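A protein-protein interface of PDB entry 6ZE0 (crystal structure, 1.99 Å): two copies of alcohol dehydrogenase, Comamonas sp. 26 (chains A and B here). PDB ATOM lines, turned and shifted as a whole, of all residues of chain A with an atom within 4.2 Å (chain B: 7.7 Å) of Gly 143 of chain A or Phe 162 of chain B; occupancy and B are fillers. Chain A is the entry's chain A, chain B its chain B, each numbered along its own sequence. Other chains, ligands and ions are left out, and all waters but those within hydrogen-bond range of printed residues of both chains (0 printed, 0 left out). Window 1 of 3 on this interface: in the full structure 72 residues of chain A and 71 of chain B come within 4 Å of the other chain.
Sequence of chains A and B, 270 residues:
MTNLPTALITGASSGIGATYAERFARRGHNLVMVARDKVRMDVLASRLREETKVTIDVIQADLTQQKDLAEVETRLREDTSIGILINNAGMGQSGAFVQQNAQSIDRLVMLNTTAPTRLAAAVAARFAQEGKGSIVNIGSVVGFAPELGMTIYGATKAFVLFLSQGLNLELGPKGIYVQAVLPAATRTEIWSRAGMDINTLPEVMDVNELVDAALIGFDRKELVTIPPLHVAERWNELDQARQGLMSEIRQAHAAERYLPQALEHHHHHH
Hydrophobic or aromatic side chains of chain B within 4 Å of the printed part of chain A: Phe 159, Phe 162, Leu 163 and Met 246.
Hydrophobic or aromatic side chains of chain A within 4 Å of the printed part of chain B: Val 141, Phe 144, Ala 145, Pro 146 and Ala 155.
The backbone carbonyl oxygen (O) of Gly 166 of chain B lies close to the side-chain hydroxyl (OG1) of Thr 151 of chain A, 3.5 Å away.
The backbone carbonyl oxygen of Phe 144 of chain A is in hydrogen-bond range of the guanidinium group of Arg 242 of chain B.
Positions printed for both chains: 157 and 158.
OG of Ser 140 of chain A sits close to N of Val 142 of chain A (3.1 Å).
Gly 143 of chain A touches one residue of chain B.
Of chain A, only Val 142, Gly 143, Ala 145, Pro 146, Thr 151, Gly 154 and Ala 155 come within 4 Å of Phe 162 of chain B.
Of the printed residues of chain A, Phe 159 of chain B touches Ala 155 (3.2 Å).
Of the printed residues of chain B, Val 142 of chain A touches Phe 162.
Of the printed residues of chain B, Val 141 of chain A touches Met 246.
Of the printed residues of chain A, Leu 163 of chain B touches Thr 151 (3.7 Å).
Of the printed residues of chain B, Ala 155 of chain A touches Phe 159 (3.2 Å) and Phe 162 (3.3 Å).
Ser 140 of chain A touches none of the printed residues of chain B.
The nearest residue of chain B that does not touch Gly 143 of chain A is Arg 242 of chain B (5.6 Å).
The nearest printed residue of chain A that does not touch Arg 242 of chain B is Ala 145 of chain A (4.2 Å).
Among the printed residues, pairs that only touch across the chains: Val 142 of chain A with Phe 162 of chain B (3.2 Å), Ala 155 of chain A with Phe 159 of chain B (3.2 Å), Ala 155 of chain A with Phe 162 of chain B (3.3 Å), Pro 146 of chain A with Arg 242 of chain B (3.3 Å), Gly 143 of chain A with Phe 162 of chain B (3.3 Å), Gly 154 of chain A with Phe 162 of chain B (3.4 Å), Pro 146 of chain A with Phe 162 of chain B (3.5 Å), Val 141 of chain A with Met 246 of chain B (3.5 Å), Thr 151 of chain A with Phe 162 of chain B (3.5 Å), Phe 144 of chain A with Met 246 of chain B (3.6 Å), Ala 145 of chain A with Met 246 of chain B (3.7 Å), Thr 151 of chain A with Leu 163 of chain B (3.7 Å), Ala 145 of chain A with Phe 162 of chain B (3.7 Å), Pro 146 of chain A with Gln 165 of chain B (3.9 Å) and Pro 146 of chain A with Gly 166 of chain B (3.9 Å).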
ATOM      1  N   SER A 140     -21.123  -8.023  10.815  1.00  0.00           N
ATOM      2  CA  SER A 140     -20.327  -8.248  12.013  1.00  0.00           C
ATOM      3  C   SER A 140     -21.228  -8.199  13.237  1.00  0.00           C
ATOM      4  O   SER A 140     -22.217  -7.462  13.272  1.00  0.00           O
ATOM      5  CB  SER A 140     -19.202  -7.217  12.154  1.00  0.00           C
ATOM      6  OG  SER A 140     -18.512  -7.366  13.386  1.00  0.00           O
ATOM      7  N   VAL A 141     -20.864  -9.002  14.240  1.00  0.00           N
ATOM      8  CA  VAL A 141     -21.529  -8.943  15.538  1.00  0.00           C
ATOM      9  C   VAL A 141     -21.379  -7.557  16.155  1.00  0.00           C
ATOM     10  O   VAL A 141     -22.249  -7.106  16.913  1.00  0.00           O
ATOM     11  CB  VAL A 141     -20.964 -10.053  16.452  1.00  0.00           C
ATOM     12  CG1 VAL A 141     -21.427  -9.884  17.880  1.00  0.00           C
ATOM     13  CG2 VAL A 141     -21.368 -11.424  15.928  1.00  0.00           C
ATOM     14  N   VAL A 142     -20.296  -6.847  15.817  1.00  0.00           N
ATOM     15  CA  VAL A 142     -20.078  -5.494  16.321  1.00  0.00           C
ATOM     16  C   VAL A 142     -21.224  -4.562  15.945  1.00  0.00           C
ATOM     17  O   VAL A 142     -21.474  -3.574  16.645  1.00  0.00           O
ATOM     18  CB  VAL A 142     -18.722  -4.956  15.810  1.00  0.00           C
ATOM     19  CG1 VAL A 142     -18.425  -3.582  16.388  1.00  0.00           C
ATOM     20  CG2 VAL A 142     -17.606  -5.926  16.159  1.00  0.00           C
ATOM     21  N   GLY A 143     -21.951  -4.869  14.869  1.00  0.00           N
ATOM     22  CA  GLY A 143     -23.136  -4.103  14.516  1.00  0.00           C
ATOM     23  C   GLY A 143     -24.225  -4.122  15.570  1.00  0.00           C
ATOM     24  O   GLY A 143     -25.175  -3.334  15.471  1.00  0.00           O
ATOM     25  N   PHE A 144     -24.109  -4.996  16.572  1.00  0.00           N
ATOM     26  CA  PHE A 144     -25.020  -5.053  17.706  1.00  0.00           C
ATOM     27  C   PHE A 144     -24.434  -4.446  18.973  1.00  0.00           C
ATOM     28  O   PHE A 144     -25.132  -4.385  19.989  1.00  0.00           O
ATOM     29  CB  PHE A 144     -25.411  -6.506  18.007  1.00  0.00           C
ATOM     30  CG  PHE A 144     -26.144  -7.196  16.895  1.00  0.00           C
ATOM     31  CD1 PHE A 144     -27.228  -6.594  16.276  1.00  0.00           C
ATOM     32  CD2 PHE A 144     -25.765  -8.464  16.487  1.00  0.00           C
ATOM     33  CE1 PHE A 144     -27.909  -7.239  15.262  1.00  0.00           C
ATOM     34  CE2 PHE A 144     -26.442  -9.113  15.475  1.00  0.00           C
ATOM     35  CZ  PHE A 144     -27.515  -8.501  14.861  1.00  0.00           C
ATOM     36  N   ALA A 145     -23.176  -4.010  18.952  1.00  0.00           N
ATOM     37  CA  ALA A 145     -22.429  -3.713  20.173  1.00  0.00           C
ATOM     38  C   ALA A 145     -21.733  -2.361  20.085  1.00  0.00           C
ATOM     39  O   ALA A 145     -20.521  -2.288  19.849  1.00  0.00           O
ATOM     40  CB  ALA A 145     -21.413  -4.819  20.462  1.00  0.00           C
ATOM     41  N   PRO A 146     -22.473  -1.264  20.275  1.00  0.00           N
ATOM     42  CA  PRO A 146     -21.805   0.035  20.455  1.00  0.00           C
ATOM     43  C   PRO A 146     -20.922   0.086  21.687  1.00  0.00           C
ATOM     44  O   PRO A 146     -20.052   0.962  21.773  1.00  0.00           O
ATOM     45  CB  PRO A 146     -22.975   1.023  20.562  1.00  0.00           C
ATOM     46  CG  PRO A 146     -24.141   0.188  20.983  1.00  0.00           C
ATOM     47  CD  PRO A 146     -23.939  -1.142  20.328  1.00  0.00           C
ATOM     48  N   THR A 151     -16.919   2.573  16.972  1.00  0.00           N
ATOM     49  CA  THR A 151     -18.166   3.253  16.634  1.00  0.00           C
ATOM     50  C   THR A 151     -18.408   3.275  15.129  1.00  0.00           C
ATOM     51  O   THR A 151     -19.488   2.896  14.661  1.00  0.00           O
ATOM     52  CB  THR A 151     -18.153   4.671  17.199  1.00  0.00           C
ATOM     53  OG1 THR A 151     -18.094   4.612  18.628  1.00  0.00           O
ATOM     54  CG2 THR A 151     -19.407   5.419  16.778  1.00  0.00           C
ATOM     55  N   GLY A 154     -18.617  -0.398  13.676  1.00  0.00           N
ATOM     56  CA  GLY A 154     -19.905  -0.960  14.047  1.00  0.00           C
ATOM     57  C   GLY A 154     -21.057  -0.313  13.303  1.00  0.00           C
ATOM     58  O   GLY A 154     -22.033  -0.980  12.951  1.00  0.00           O
ATOM     59  N   ALA A 155     -20.960   0.995  13.053  1.00  0.00           N
ATOM     60  CA  ALA A 155     -22.020   1.686  12.324  1.00  0.00           C
ATOM     61  C   ALA A 155     -22.114   1.194  10.884  1.00  0.00           C
ATOM     62  O   ALA A 155     -23.220   1.013  10.359  1.00  0.00           O
ATOM     63  CB  ALA A 155     -21.791   3.196  12.371  1.00  0.00           C
ATOM     64  N   LYS A 157     -21.386  -1.755   9.905  1.00  0.00           N
ATOM     65  CA  LYS A 157     -21.925  -3.108   9.942  1.00  0.00           C
ATOM     66  C   LYS A 157     -23.414  -3.130  10.266  1.00  0.00           C
ATOM     67  O   LYS A 157     -24.126  -4.032   9.809  1.00  0.00           O
ATOM     68  CB  LYS A 157     -21.140  -3.947  10.949  1.00  0.00           C
ATOM     69  CG  LYS A 157     -19.694  -4.153  10.536  1.00  0.00           C
ATOM     70  CD  LYS A 157     -19.625  -4.685   9.115  1.00  0.00           C
ATOM     71  CE  LYS A 157     -18.194  -4.912   8.671  1.00  0.00           C
ATOM     72  NZ  LYS A 157     -18.146  -5.468   7.294  1.00  0.00           N
ATOM     73  N   ALA A 158     -23.904  -2.161  11.043  1.00  0.00           N
ATOM     74  CA  ALA A 158     -25.347  -2.003  11.190  1.00  0.00           C
ATOM     75  C   ALA A 158     -25.982  -1.647   9.853  1.00  0.00           C
ATOM     76  O   ALA A 158     -27.081  -2.115   9.532  1.00  0.00           O
ATOM     77  CB  ALA A 158     -25.660  -0.942  12.243  1.00  0.00           C
ATOM     78  N   ASN B 137     -27.820  14.155  16.284  1.00  0.00           N
ATOM     79  CA  ASN B 137     -27.878  13.441  15.014  1.00  0.00           C
ATOM     80  C   ASN B 137     -29.328  13.153  14.664  1.00  0.00           C
ATOM     81  O   ASN B 137     -30.068  12.586  15.476  1.00  0.00           O
ATOM     82  CB  ASN B 137     -27.088  12.133  15.075  1.00  0.00           C
ATOM     83  CG  ASN B 137     -25.615  12.356  15.323  1.00  0.00           C
ATOM     84  OD1 ASN B 137     -25.011  13.261  14.751  1.00  0.00           O
ATOM     85  ND2 ASN B 137     -25.024  11.527  16.177  1.00  0.00           N
ATOM     86  N   THR B 156     -28.678   3.885   5.972  1.00  0.00           N
ATOM     87  CA  THR B 156     -27.920   5.039   6.454  1.00  0.00           C
ATOM     88  C   THR B 156     -28.446   5.524   7.797  1.00  0.00           C
ATOM     89  O   THR B 156     -27.672   6.008   8.631  1.00  0.00           O
ATOM     90  CB  THR B 156     -27.962   6.183   5.437  1.00  0.00           C
ATOM     91  OG1 THR B 156     -29.307   6.668   5.305  1.00  0.00           O
ATOM     92  CG2 THR B 156     -27.454   5.718   4.079  1.00  0.00           C
ATOM     93  N   LYS B 157     -29.752   5.402   8.029  1.00  0.00           N
ATOM     94  CA  LYS B 157     -30.314   5.829   9.302  1.00  0.00           C
ATOM     95  C   LYS B 157     -30.045   4.815  10.406  1.00  0.00           C
ATOM     96  O   LYS B 157     -29.950   5.195  11.580  1.00  0.00           O
ATOM     97  CB  LYS B 157     -31.809   6.100   9.144  1.00  0.00           C
ATOM     98  CG  LYS B 157     -32.083   7.275   8.219  1.00  0.00           C
ATOM     99  CD  LYS B 157     -31.263   8.485   8.657  1.00  0.00           C
ATOM    100  CE  LYS B 157     -31.506   9.694   7.772  1.00  0.00           C
ATOM    101  NZ  LYS B 157     -30.720  10.873   8.239  1.00  0.00           N
ATOM    102  N   ALA B 158     -29.930   3.532  10.060  1.00  0.00           N
ATOM    103  CA  ALA B 158     -29.421   2.560  11.021  1.00  0.00           C
ATOM    104  C   ALA B 158     -27.980   2.882  11.393  1.00  0.00           C
ATOM    105  O   ALA B 158     -27.587   2.762  12.560  1.00  0.00           O
ATOM    106  CB  ALA B 158     -29.527   1.145  10.453  1.00  0.00           C
ATOM    107  N   PHE B 159     -27.181   3.295  10.404  1.00  0.00           N
ATOM    108  CA  PHE B 159     -25.832   3.786  10.668  1.00  0.00           C
ATOM    109  C   PHE B 159     -25.851   4.934  11.670  1.00  0.00           C
ATOM    110  O   PHE B 159     -25.092   4.934  12.647  1.00  0.00           O
ATOM    111  CB  PHE B 159     -25.175   4.227   9.352  1.00  0.00           C
ATOM    112  CG  PHE B 159     -23.747   4.704   9.498  1.00  0.00           C
ATOM    113  CD1 PHE B 159     -23.460   5.951  10.041  1.00  0.00           C
ATOM    114  CD2 PHE B 159     -22.695   3.917   9.059  1.00  0.00           C
ATOM    115  CE1 PHE B 159     -22.153   6.388  10.174  1.00  0.00           C
ATOM    116  CE2 PHE B 159     -21.383   4.349   9.182  1.00  0.00           C
ATOM    117  CZ  PHE B 159     -21.112   5.585   9.743  1.00  0.00           C
ATOM    118  N   VAL B 160     -26.712   5.929  11.437  1.00  0.00           N
ATOM    119  CA  VAL B 160     -26.694   7.142  12.252  1.00  0.00           C
ATOM    120  C   VAL B 160     -27.047   6.819  13.698  1.00  0.00           C
ATOM    121  O   VAL B 160     -26.448   7.363  14.635  1.00  0.00           O
ATOM    122  CB  VAL B 160     -27.638   8.203  11.653  1.00  0.00           C
ATOM    123  CG1 VAL B 160     -27.821   9.368  12.614  1.00  0.00           C
ATOM    124  CG2 VAL B 160     -27.096   8.693  10.323  1.00  0.00           C
ATOM    125  N   LEU B 161     -28.014   5.922  13.905  1.00  0.00           N
ATOM    126  CA  LEU B 161     -28.377   5.542  15.265  1.00  0.00           C
ATOM    127  C   LEU B 161     -27.216   4.856  15.972  1.00  0.00           C
ATOM    128  O   LEU B 161     -26.927   5.154  17.137  1.00  0.00           O
ATOM    129  CB  LEU B 161     -29.612   4.640  15.256  1.00  0.00           C
ATOM    130  CG  LEU B 161     -30.032   4.113  16.630  1.00  0.00           C
ATOM    131  CD1 LEU B 161     -30.292   5.260  17.598  1.00  0.00           C
ATOM    132  CD2 LEU B 161     -31.257   3.219  16.512  1.00  0.00           C
ATOM    133  N   PHE B 162     -26.546   3.922  15.290  1.00  0.00           N
ATOM    134  CA  PHE B 162     -25.391   3.270  15.899  1.00  0.00           C
ATOM    135  C   PHE B 162     -24.302   4.286  16.213  1.00  0.00           C
ATOM    136  O   PHE B 162     -23.683   4.232  17.282  1.00  0.00           O
ATOM    137  CB  PHE B 162     -24.847   2.174  14.984  1.00  0.00           C
ATOM    138  CG  PHE B 162     -23.865   1.257  15.659  1.00  0.00           C
ATOM    139  CD1 PHE B 162     -24.260   0.002  16.096  1.00  0.00           C
ATOM    140  CD2 PHE B 162     -22.550   1.651  15.874  1.00  0.00           C
ATOM    141  CE1 PHE B 162     -23.362  -0.845  16.724  1.00  0.00           C
ATOM    142  CE2 PHE B 162     -21.651   0.811  16.506  1.00  0.00           C
ATOM    143  CZ  PHE B 162     -22.057  -0.440  16.929  1.00  0.00           C
ATOM    144  N   LEU B 163     -24.052   5.214  15.287  1.00  0.00           N
ATOM    145  CA  LEU B 163     -23.076   6.273  15.527  1.00  0.00           C
ATOM    146  C   LEU B 163     -23.403   7.038  16.804  1.00  0.00           C
ATOM    147  O   LEU B 163     -22.524   7.278  17.640  1.00  0.00           O
ATOM    148  CB  LEU B 163     -23.030   7.219  14.326  1.00  0.00           C
ATOM    149  CG  LEU B 163     -22.070   8.405  14.414  1.00  0.00           C
ATOM    150  CD1 LEU B 163     -20.631   7.924  14.360  1.00  0.00           C
ATOM    151  CD2 LEU B 163     -22.347   9.405  13.304  1.00  0.00           C
ATOM    152  N   SER B 164     -24.673   7.419  16.976  1.00  0.00           N
ATOM    153  CA  SER B 164     -25.079   8.144  18.176  1.00  0.00           C
ATOM    154  C   SER B 164     -24.831   7.315  19.432  1.00  0.00           C
ATOM    155  O   SER B 164     -24.313   7.824  20.434  1.00  0.00           O
ATOM    156  CB  SER B 164     -26.555   8.532  18.076  1.00  0.00           C
ATOM    157  OG  SER B 164     -26.800   9.314  16.924  1.00  0.00           O
ATOM    158  N   GLN B 165     -25.199   6.032  19.396  1.00  0.00           N
ATOM    159  CA  GLN B 165     -24.982   5.168  20.553  1.00  0.00           C
ATOM    160  C   GLN B 165     -23.497   5.002  20.847  1.00  0.00           C
ATOM    161  O   GLN B 165     -23.083   5.004  22.013  1.00  0.00           O
ATOM    162  CB  GLN B 165     -25.637   3.806  20.320  1.00  0.00           C
ATOM    163  CG  GLN B 165     -27.158   3.842  20.294  1.00  0.00           C
ATOM    164  CD  GLN B 165     -27.761   2.514  19.879  1.00  0.00           C
ATOM    165  OE1 GLN B 165     -27.543   2.045  18.764  1.00  0.00           O
ATOM    166  NE2 GLN B 165     -28.521   1.902  20.777  1.00  0.00           N
ATOM    167  N   GLY B 166     -22.681   4.842  19.804  1.00  0.00           N
ATOM    168  CA  GLY B 166     -21.249   4.719  20.013  1.00  0.00           C
ATOM    169  C   GLY B 166     -20.624   5.994  20.543  1.00  0.00           C
ATOM    170  O   GLY B 166     -19.714   5.952  21.374  1.00  0.00           O
ATOM    171  N   LEU B 167     -21.097   7.146  20.064  1.00  0.00           N
ATOM    172  CA  LEU B 167     -20.515   8.413  20.494  1.00  0.00           C
ATOM    173  C   LEU B 167     -20.881   8.739  21.938  1.00  0.00           C
ATOM    174  O   LEU B 167     -20.058   9.293  22.676  1.00  0.00           O
ATOM    175  CB  LEU B 167     -20.944   9.538  19.553  1.00  0.00           C
ATOM    176  CG  LEU B 167     -20.292   9.476  18.170  1.00  0.00           C
ATOM    177  CD1 LEU B 167     -20.591  10.730  17.363  1.00  0.00           C
ATOM    178  CD2 LEU B 167     -18.793   9.266  18.312  1.00  0.00           C
ATOM    179  N   ASN B 168     -22.106   8.415  22.358  1.00  0.00           N
ATOM    180  CA  ASN B 168     -22.490   8.635  23.750  1.00  0.00           C
ATOM    181  C   ASN B 168     -21.565   7.889  24.702  1.00  0.00           C
ATOM    182  O   ASN B 168     -21.082   8.455  25.687  1.00  0.00           O
ATOM    183  CB  ASN B 168     -23.941   8.210  23.980  1.00  0.00           C
ATOM    184  CG  ASN B 168     -24.276   8.072  25.458  1.00  0.00           C
ATOM    185  OD1 ASN B 168     -24.563   6.976  25.939  1.00  0.00           O
ATOM    186  ND2 ASN B 168     -24.216   9.180  26.189  1.00  0.00           N
ATOM    187  N   ALA B 180     -29.779  11.184  19.729  1.00  0.00           N
ATOM    188  CA  ALA B 180     -30.326  10.668  18.484  1.00  0.00           C
ATOM    189  C   ALA B 180     -31.801  11.043  18.411  1.00  0.00           C
ATOM    190  O   ALA B 180     -32.589  10.643  19.274  1.00  0.00           O
ATOM    191  CB  ALA B 180     -30.148   9.152  18.389  1.00  0.00           C
ATOM    192  N   ARG B 242     -31.211  -6.255  22.159  1.00  0.00           N
ATOM    193  CA  ARG B 242     -29.909  -6.129  21.508  1.00  0.00           C
ATOM    194  C   ARG B 242     -28.791  -6.633  22.411  1.00  0.00           C
ATOM    195  O   ARG B 242     -27.988  -7.484  22.012  1.00  0.00           O
ATOM    196  CB  ARG B 242     -29.659  -4.674  21.109  1.00  0.00           C
ATOM    197  CG  ARG B 242     -28.296  -4.447  20.474  1.00  0.00           C
ATOM    198  CD  ARG B 242     -27.999  -2.969  20.248  1.00  0.00           C
ATOM    199  NE  ARG B 242     -28.021  -2.199  21.489  1.00  0.00           N
ATOM    200  CZ  ARG B 242     -27.048  -2.204  22.396  1.00  0.00           C
ATOM    201  NH1 ARG B 242     -25.968  -2.954  22.214  1.00  0.00           N
ATOM    202  NH2 ARG B 242     -27.159  -1.464  23.492  1.00  0.00           N
ATOM    203  N   MET B 246     -26.142 -10.003  22.467  1.00  0.00           N
ATOM    204  CA  MET B 246     -24.704  -9.927  22.700  1.00  0.00           C
ATOM    205  C   MET B 246     -24.282 -10.793  23.878  1.00  0.00           C
ATOM    206  O   MET B 246     -23.160 -11.312  23.900  1.00  0.00           O
ATOM    207  CB  MET B 246     -24.283  -8.476  22.938  1.00  0.00           C
ATOM    208  CG  MET B 246     -24.336  -7.610  21.694  1.00  0.00           C
ATOM    209  SD  MET B 246     -23.295  -8.274  20.383  1.00  0.00           S
ATOM    210  CE  MET B 246     -21.716  -8.382  21.227  1.00  0.00           C
